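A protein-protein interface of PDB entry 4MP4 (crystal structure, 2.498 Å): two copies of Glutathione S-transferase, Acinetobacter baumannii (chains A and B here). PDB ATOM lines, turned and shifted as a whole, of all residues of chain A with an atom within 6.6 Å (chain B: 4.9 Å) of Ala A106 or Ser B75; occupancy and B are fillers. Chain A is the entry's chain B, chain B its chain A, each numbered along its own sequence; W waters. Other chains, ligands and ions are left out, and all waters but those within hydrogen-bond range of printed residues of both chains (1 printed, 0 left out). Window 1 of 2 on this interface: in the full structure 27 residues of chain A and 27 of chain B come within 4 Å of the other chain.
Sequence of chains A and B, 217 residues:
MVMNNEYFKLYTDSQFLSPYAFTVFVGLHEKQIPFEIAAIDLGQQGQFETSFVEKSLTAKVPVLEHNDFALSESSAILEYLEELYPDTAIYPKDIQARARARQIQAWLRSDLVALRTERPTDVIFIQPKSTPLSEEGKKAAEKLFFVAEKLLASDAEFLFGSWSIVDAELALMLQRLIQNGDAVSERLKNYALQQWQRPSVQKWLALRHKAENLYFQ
Along chain A the printed residues that touch a printed residue of chain B span positions 102 to 107.
Of the 8 printed residues of chain B, 4 touch a printed residue of chain A.
Hydrophobic or aromatic side chains of chain B within 4 Å of the printed part of chain A: Ala B76.
Along chain B the printed residues that touch a printed residue of chain A span positions 73 to 79.
Among the printed residues, 7 pairs touch across the chains.
Among the printed residues, no Asp or Glu carboxylate lies within 4 Å of a Lys or Arg side-chain nitrogen of the other chain.
The indole nitrogen of Trp A107 lies within hydrogen-bond range of the side-chain carboxylate of Asp A111 (3.3 Å).
Water W1 bridges NH1 of Arg A102 and O of Ala B76.
Of the printed residues of chain B, Arg A102 touches Ala B76 and Glu B79.
Printed residues of chain B within 4 Å of Gln A103: Glu B73 and Ala B76.
Ile A104 touches none of the printed residues of chain B.
Of the printed residues of chain B, Ala A106 touches Glu B73 and Ser B75.
Ser A110 touches none of the printed residues of chain B.
Printed residues of chain A within 4 Å of Glu B73: Gln A103, Ala A106 and Trp A107.
Printed residues of chain A within 4 Å of Ser B75: Ala A106.
Of the printed residues of chain A, Ala B76 touches Arg A102 (3.8 Å) and Gln A103 (3.6 Å).
The nearest printed residue of chain B that does not touch Ala A106 is Ala B76 (5.3 Å).
Among the printed residues, merely in contact across the chains: Arg A102 with Ala B76 (3.8 Å), Arg A102 with Glu B79 (3.4 Å), Gln A103 with Glu B73 (3.5 Å), Gln A103 with Ala B76 (3.6 Å), Ala A106 with Glu B73 (3.8 Å), Ala A106 with Ser B75 (3.99 Å) and Trp A107 with Glu B73 (3.3 Å).
Positions printed for both chains: 75 and 105.
Of the 7 pairs that touch across the chains among the printed residues, none has its exchanged pair printed and touching as well.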
ATOM      1  N   SER A  75      32.023 -15.477  -0.849  1.00  0.00           N
ATOM      2  CA  SER A  75      32.066 -14.191  -1.563  1.00  0.00           C
ATOM      3  C   SER A  75      33.345 -13.409  -1.243  1.00  0.00           C
ATOM      4  O   SER A  75      33.969 -12.847  -2.136  1.00  0.00           O
ATOM      5  CB  SER A  75      30.820 -13.339  -1.293  1.00  0.00           C
ATOM      6  OG  SER A  75      30.694 -12.997   0.082  1.00  0.00           O
ATOM      7  N   ALA A 101      26.056  -9.089 -11.156  1.00  0.00           N
ATOM      8  CA  ALA A 101      26.636 -10.376 -10.798  1.00  0.00           C
ATOM      9  C   ALA A 101      26.734 -10.515  -9.275  1.00  0.00           C
ATOM     10  O   ALA A 101      26.260 -11.503  -8.708  1.00  0.00           O
ATOM     11  CB  ALA A 101      28.001 -10.578 -11.463  1.00  0.00           C
ATOM     12  N   ARG A 102      27.319  -9.514  -8.618  1.00  0.00           N
ATOM     13  CA  ARG A 102      27.429  -9.528  -7.158  1.00  0.00           C
ATOM     14  C   ARG A 102      26.060  -9.567  -6.500  1.00  0.00           C
ATOM     15  O   ARG A 102      25.872 -10.239  -5.509  1.00  0.00           O
ATOM     16  CB  ARG A 102      28.250  -8.351  -6.641  1.00  0.00           C
ATOM     17  CG  ARG A 102      29.756  -8.478  -6.894  1.00  0.00           C
ATOM     18  CD  ARG A 102      30.524  -7.390  -6.159  1.00  0.00           C
ATOM     19  NE  ARG A 102      31.962  -7.400  -6.406  1.00  0.00           N
ATOM     20  CZ  ARG A 102      32.599  -6.521  -7.176  1.00  0.00           C
ATOM     21  NH1 ARG A 102      31.926  -5.554  -7.792  1.00  0.00           N
ATOM     22  NH2 ARG A 102      33.912  -6.605  -7.335  1.00  0.00           N
ATOM     23  N   GLN A 103      25.093  -8.881  -7.087  1.00  0.00           N
ATOM     24  CA  GLN A 103      23.712  -8.936  -6.599  1.00  0.00           C
ATOM     25  C   GLN A 103      23.121 -10.353  -6.617  1.00  0.00           C
ATOM     26  O   GLN A 103      22.615 -10.844  -5.591  1.00  0.00           O
ATOM     27  CB  GLN A 103      22.829  -8.011  -7.424  1.00  0.00           C
ATOM     28  CG  GLN A 103      21.377  -7.975  -6.989  1.00  0.00           C
ATOM     29  CD  GLN A 103      20.506  -7.219  -7.990  1.00  0.00           C
ATOM     30  OE1 GLN A 103      20.980  -6.317  -8.692  1.00  0.00           O
ATOM     31  NE2 GLN A 103      19.231  -7.587  -8.064  1.00  0.00           N
ATOM     32  N   ILE A 104      23.184 -11.005  -7.780  1.00  0.00           N
ATOM     33  CA  ILE A 104      22.554 -12.304  -7.926  1.00  0.00           C
ATOM     34  C   ILE A 104      23.237 -13.275  -6.987  1.00  0.00           C
ATOM     35  O   ILE A 104      22.574 -14.071  -6.298  1.00  0.00           O
ATOM     36  CB  ILE A 104      22.557 -12.826  -9.390  1.00  0.00           C
ATOM     37  CG1 ILE A 104      21.864 -11.832 -10.313  1.00  0.00           C
ATOM     38  CG2 ILE A 104      21.864 -14.176  -9.466  1.00  0.00           C
ATOM     39  CD1 ILE A 104      20.447 -11.451  -9.848  1.00  0.00           C
ATOM     40  N   GLN A 105      24.561 -13.158  -6.914  1.00  0.00           N
ATOM     41  CA  GLN A 105      25.353 -13.970  -5.986  1.00  0.00           C
ATOM     42  C   GLN A 105      24.929 -13.766  -4.508  1.00  0.00           C
ATOM     43  O   GLN A 105      24.894 -14.725  -3.731  1.00  0.00           O
ATOM     44  CB  GLN A 105      26.856 -13.701  -6.194  1.00  0.00           C
ATOM     45  CG  GLN A 105      27.808 -14.337  -5.173  1.00  0.00           C
ATOM     46  CD  GLN A 105      29.268 -14.065  -5.511  1.00  0.00           C
ATOM     47  OE1 GLN A 105      29.871 -14.753  -6.341  1.00  0.00           O
ATOM     48  NE2 GLN A 105      29.839 -13.042  -4.889  1.00  0.00           N
ATOM     49  N   ALA A 106      24.593 -12.532  -4.129  1.00  0.00           N
ATOM     50  CA  ALA A 106      24.265 -12.237  -2.735  1.00  0.00           C
ATOM     51  C   ALA A 106      22.883 -12.754  -2.419  1.00  0.00           C
ATOM     52  O   ALA A 106      22.635 -13.300  -1.342  1.00  0.00           O
ATOM     53  CB  ALA A 106      24.353 -10.741  -2.448  1.00  0.00           C
ATOM     54  N   TRP A 107      22.001 -12.590  -3.392  1.00  0.00           N
ATOM     55  CA  TRP A 107      20.629 -13.043  -3.303  1.00  0.00           C
ATOM     56  C   TRP A 107      20.554 -14.566  -3.176  1.00  0.00           C
ATOM     57  O   TRP A 107      19.822 -15.092  -2.329  1.00  0.00           O
ATOM     58  CB  TRP A 107      19.870 -12.528  -4.532  1.00  0.00           C
ATOM     59  CG  TRP A 107      18.495 -13.051  -4.708  1.00  0.00           C
ATOM     60  CD1 TRP A 107      17.383 -12.711  -3.987  1.00  0.00           C
ATOM     61  CD2 TRP A 107      18.064 -13.990  -5.697  1.00  0.00           C
ATOM     62  NE1 TRP A 107      16.286 -13.398  -4.460  1.00  0.00           N
ATOM     63  CE2 TRP A 107      16.675 -14.185  -5.509  1.00  0.00           C
ATOM     64  CE3 TRP A 107      18.715 -14.689  -6.719  1.00  0.00           C
ATOM     65  CZ2 TRP A 107      15.929 -15.051  -6.309  1.00  0.00           C
ATOM     66  CZ3 TRP A 107      17.974 -15.552  -7.511  1.00  0.00           C
ATOM     67  CH2 TRP A 107      16.593 -15.721  -7.306  1.00  0.00           C
ATOM     68  N   LEU A 108      21.325 -15.280  -3.993  1.00  0.00           N
ATOM     69  CA  LEU A 108      21.341 -16.743  -3.913  1.00  0.00           C
ATOM     70  C   LEU A 108      21.922 -17.214  -2.582  1.00  0.00           C
ATOM     71  O   LEU A 108      21.600 -18.300  -2.094  1.00  0.00           O
ATOM     72  CB  LEU A 108      22.132 -17.365  -5.073  1.00  0.00           C
ATOM     73  CG  LEU A 108      21.592 -17.306  -6.510  1.00  0.00           C
ATOM     74  CD1 LEU A 108      22.751 -17.516  -7.489  1.00  0.00           C
ATOM     75  CD2 LEU A 108      20.475 -18.336  -6.765  1.00  0.00           C
ATOM     76  N   ARG A 109      22.791 -16.407  -1.988  1.00  0.00           N
ATOM     77  CA  ARG A 109      23.355 -16.772  -0.691  1.00  0.00           C
ATOM     78  C   ARG A 109      22.330 -16.688   0.444  1.00  0.00           C
ATOM     79  O   ARG A 109      22.293 -17.554   1.319  1.00  0.00           O
ATOM     80  CB  ARG A 109      24.540 -15.882  -0.372  1.00  0.00           C
ATOM     81  CG  ARG A 109      25.094 -16.075   1.002  1.00  0.00           C
ATOM     82  CD  ARG A 109      25.732 -17.429   1.128  1.00  0.00           C
ATOM     83  NE  ARG A 109      26.166 -17.689   2.495  1.00  0.00           N
ATOM     84  CZ  ARG A 109      25.383 -18.213   3.428  1.00  0.00           C
ATOM     85  NH1 ARG A 109      24.130 -18.527   3.135  1.00  0.00           N
ATOM     86  NH2 ARG A 109      25.853 -18.426   4.648  1.00  0.00           N
ATOM     87  N   SER A 110      21.483 -15.654   0.404  1.00  0.00           N
ATOM     88  CA  SER A 110      20.628 -15.307   1.540  1.00  0.00           C
ATOM     89  C   SER A 110      19.140 -15.565   1.360  1.00  0.00           C
ATOM     90  O   SER A 110      18.463 -15.908   2.321  1.00  0.00           O
ATOM     91  CB  SER A 110      20.852 -13.855   1.940  1.00  0.00           C
ATOM     92  OG  SER A 110      22.191 -13.679   2.367  1.00  0.00           O
ATOM     93  N   ASP A 111      18.624 -15.399   0.149  1.00  0.00           N
ATOM     94  CA  ASP A 111      17.201 -15.615  -0.078  1.00  0.00           C
ATOM     95  C   ASP A 111      16.957 -17.105  -0.352  1.00  0.00           C
ATOM     96  O   ASP A 111      17.739 -17.951   0.088  1.00  0.00           O
ATOM     97  CB  ASP A 111      16.685 -14.735  -1.223  1.00  0.00           C
ATOM     98  CG  ASP A 111      15.173 -14.495  -1.159  1.00  0.00           C
ATOM     99  OD1 ASP A 111      14.426 -15.403  -0.719  1.00  0.00           O
ATOM    100  OD2 ASP A 111      14.731 -13.393  -1.561  1.00  0.00           O
ATOM    101  N   GLU A 169      27.149 -20.903  -9.642  1.00  0.00           N
ATOM    102  CA  GLU A 169      26.307 -20.704  -8.474  1.00  0.00           C
ATOM    103  C   GLU A 169      24.814 -20.887  -8.819  1.00  0.00           C
ATOM    104  O   GLU A 169      24.075 -21.549  -8.085  1.00  0.00           O
ATOM    105  CB  GLU A 169      26.552 -19.319  -7.865  1.00  0.00           C
ATOM    106  CG  GLU A 169      27.993 -19.001  -7.529  1.00  0.00           C
ATOM    107  CD  GLU A 169      28.179 -17.555  -7.057  1.00  0.00           C
ATOM    108  OE1 GLU A 169      27.506 -16.657  -7.594  1.00  0.00           O
ATOM    109  OE2 GLU A 169      28.980 -17.314  -6.135  1.00  0.00           O
ATOM    110  N   GLU B  73      20.699  -5.624  -3.046  1.00  0.00           N
ATOM    111  CA  GLU B  73      21.665  -6.300  -2.145  1.00  0.00           C
ATOM    112  C   GLU B  73      22.766  -5.355  -1.640  1.00  0.00           C
ATOM    113  O   GLU B  73      23.586  -4.872  -2.436  1.00  0.00           O
ATOM    114  CB  GLU B  73      22.270  -7.574  -2.769  1.00  0.00           C
ATOM    115  CG  GLU B  73      21.241  -8.568  -3.322  1.00  0.00           C
ATOM    116  CD  GLU B  73      20.464  -9.294  -2.236  1.00  0.00           C
ATOM    117  OE1 GLU B  73      20.877  -9.257  -1.056  1.00  0.00           O
ATOM    118  OE2 GLU B  73      19.440  -9.923  -2.564  1.00  0.00           O
ATOM    119  N   SER B  74      22.785  -5.087  -0.329  1.00  0.00           N
ATOM    120  CA  SER B  74      23.693  -4.078   0.212  1.00  0.00           C
ATOM    121  C   SER B  74      25.180  -4.293  -0.083  1.00  0.00           C
ATOM    122  O   SER B  74      25.882  -3.343  -0.422  1.00  0.00           O
ATOM    123  CB  SER B  74      23.451  -3.818   1.708  1.00  0.00           C
ATOM    124  OG  SER B  74      23.562  -4.994   2.493  1.00  0.00           O
ATOM    125  N   SER B  75      25.671  -5.523   0.038  1.00  0.00           N
ATOM    126  CA  SER B  75      27.093  -5.764  -0.227  1.00  0.00           C
ATOM    127  C   SER B  75      27.439  -5.458  -1.678  1.00  0.00           C
ATOM    128  O   SER B  75      28.509  -4.911  -1.968  1.00  0.00           O
ATOM    129  CB  SER B  75      27.498  -7.186   0.116  1.00  0.00           C
ATOM    130  OG  SER B  75      26.623  -8.095  -0.517  1.00  0.00           O
ATOM    131  N   ALA B  76      26.528  -5.817  -2.579  1.00  0.00           N
ATOM    132  CA  ALA B  76      26.685  -5.529  -3.994  1.00  0.00           C
ATOM    133  C   ALA B  76      26.693  -4.025  -4.201  1.00  0.00           C
ATOM    134  O   ALA B  76      27.551  -3.496  -4.907  1.00  0.00           O
ATOM    135  CB  ALA B  76      25.557  -6.160  -4.793  1.00  0.00           C
ATOM    136  N   ILE B  77      25.726  -3.338  -3.589  1.00  0.00           N
ATOM    137  CA  ILE B  77      25.607  -1.895  -3.748  1.00  0.00           C
ATOM    138  C   ILE B  77      26.862  -1.184  -3.252  1.00  0.00           C
ATOM    139  O   ILE B  77      27.398  -0.313  -3.946  1.00  0.00           O
ATOM    140  CB  ILE B  77      24.339  -1.334  -3.054  1.00  0.00           C
ATOM    141  CG1 ILE B  77      23.083  -1.747  -3.834  1.00  0.00           C
ATOM    142  CG2 ILE B  77      24.399   0.182  -2.957  1.00  0.00           C
ATOM    143  CD1 ILE B  77      21.789  -1.537  -3.086  1.00  0.00           C
ATOM    144  N   LEU B  78      27.347  -1.579  -2.075  1.00  0.00           N
ATOM    145  CA  LEU B  78      28.563  -0.985  -1.515  1.00  0.00           C
ATOM    146  C   LEU B  78      29.775  -1.174  -2.437  1.00  0.00           C
ATOM    147  O   LEU B  78      30.487  -0.210  -2.757  1.00  0.00           O
ATOM    148  CB  LEU B  78      28.859  -1.540  -0.110  1.00  0.00           C
ATOM    149  CG  LEU B  78      27.913  -1.072   0.993  1.00  0.00           C
ATOM    150  CD1 LEU B  78      27.995  -1.958   2.218  1.00  0.00           C
ATOM    151  CD2 LEU B  78      28.220   0.371   1.350  1.00  0.00           C
ATOM    152  N   GLU B  79      29.984  -2.416  -2.867  1.00  0.00           N
ATOM    153  CA  GLU B  79      31.074  -2.761  -3.770  1.00  0.00           C
ATOM    154  C   GLU B  79      31.034  -1.873  -5.020  1.00  0.00           C
ATOM    155  O   GLU B  79      32.062  -1.385  -5.509  1.00  0.00           O
ATOM    156  CB  GLU B  79      30.977  -4.242  -4.144  1.00  0.00           C
ATOM    157  CG  GLU B  79      32.289  -4.997  -4.061  1.00  0.00           C
ATOM    158  CD  GLU B  79      32.670  -5.371  -2.646  1.00  0.00           C
ATOM    159  OE1 GLU B  79      32.234  -6.445  -2.188  1.00  0.00           O
ATOM    160  OE2 GLU B  79      33.416  -4.610  -1.995  1.00  0.00           O
ATOM    161  N   GLN B 105      31.498  -8.828   7.275  1.00  0.00           N
ATOM    162  CA  GLN B 105      30.280  -8.392   6.592  1.00  0.00           C
ATOM    163  C   GLN B 105      29.421  -9.559   6.047  1.00  0.00           C
ATOM    164  O   GLN B 105      28.195  -9.543   6.182  1.00  0.00           O
ATOM    165  CB  GLN B 105      30.638  -7.440   5.452  1.00  0.00           C
ATOM    166  CG  GLN B 105      29.450  -6.804   4.781  1.00  0.00           C
ATOM    167  CD  GLN B 105      29.863  -5.825   3.698  1.00  0.00           C
ATOM    168  OE1 GLN B 105      30.333  -6.222   2.633  1.00  0.00           O
ATOM    169  NE2 GLN B 105      29.694  -4.541   3.966  1.00  0.00           N
HETATM  170  O   HOH W   1      29.260  -4.679  -7.309  1.00  0.00           O
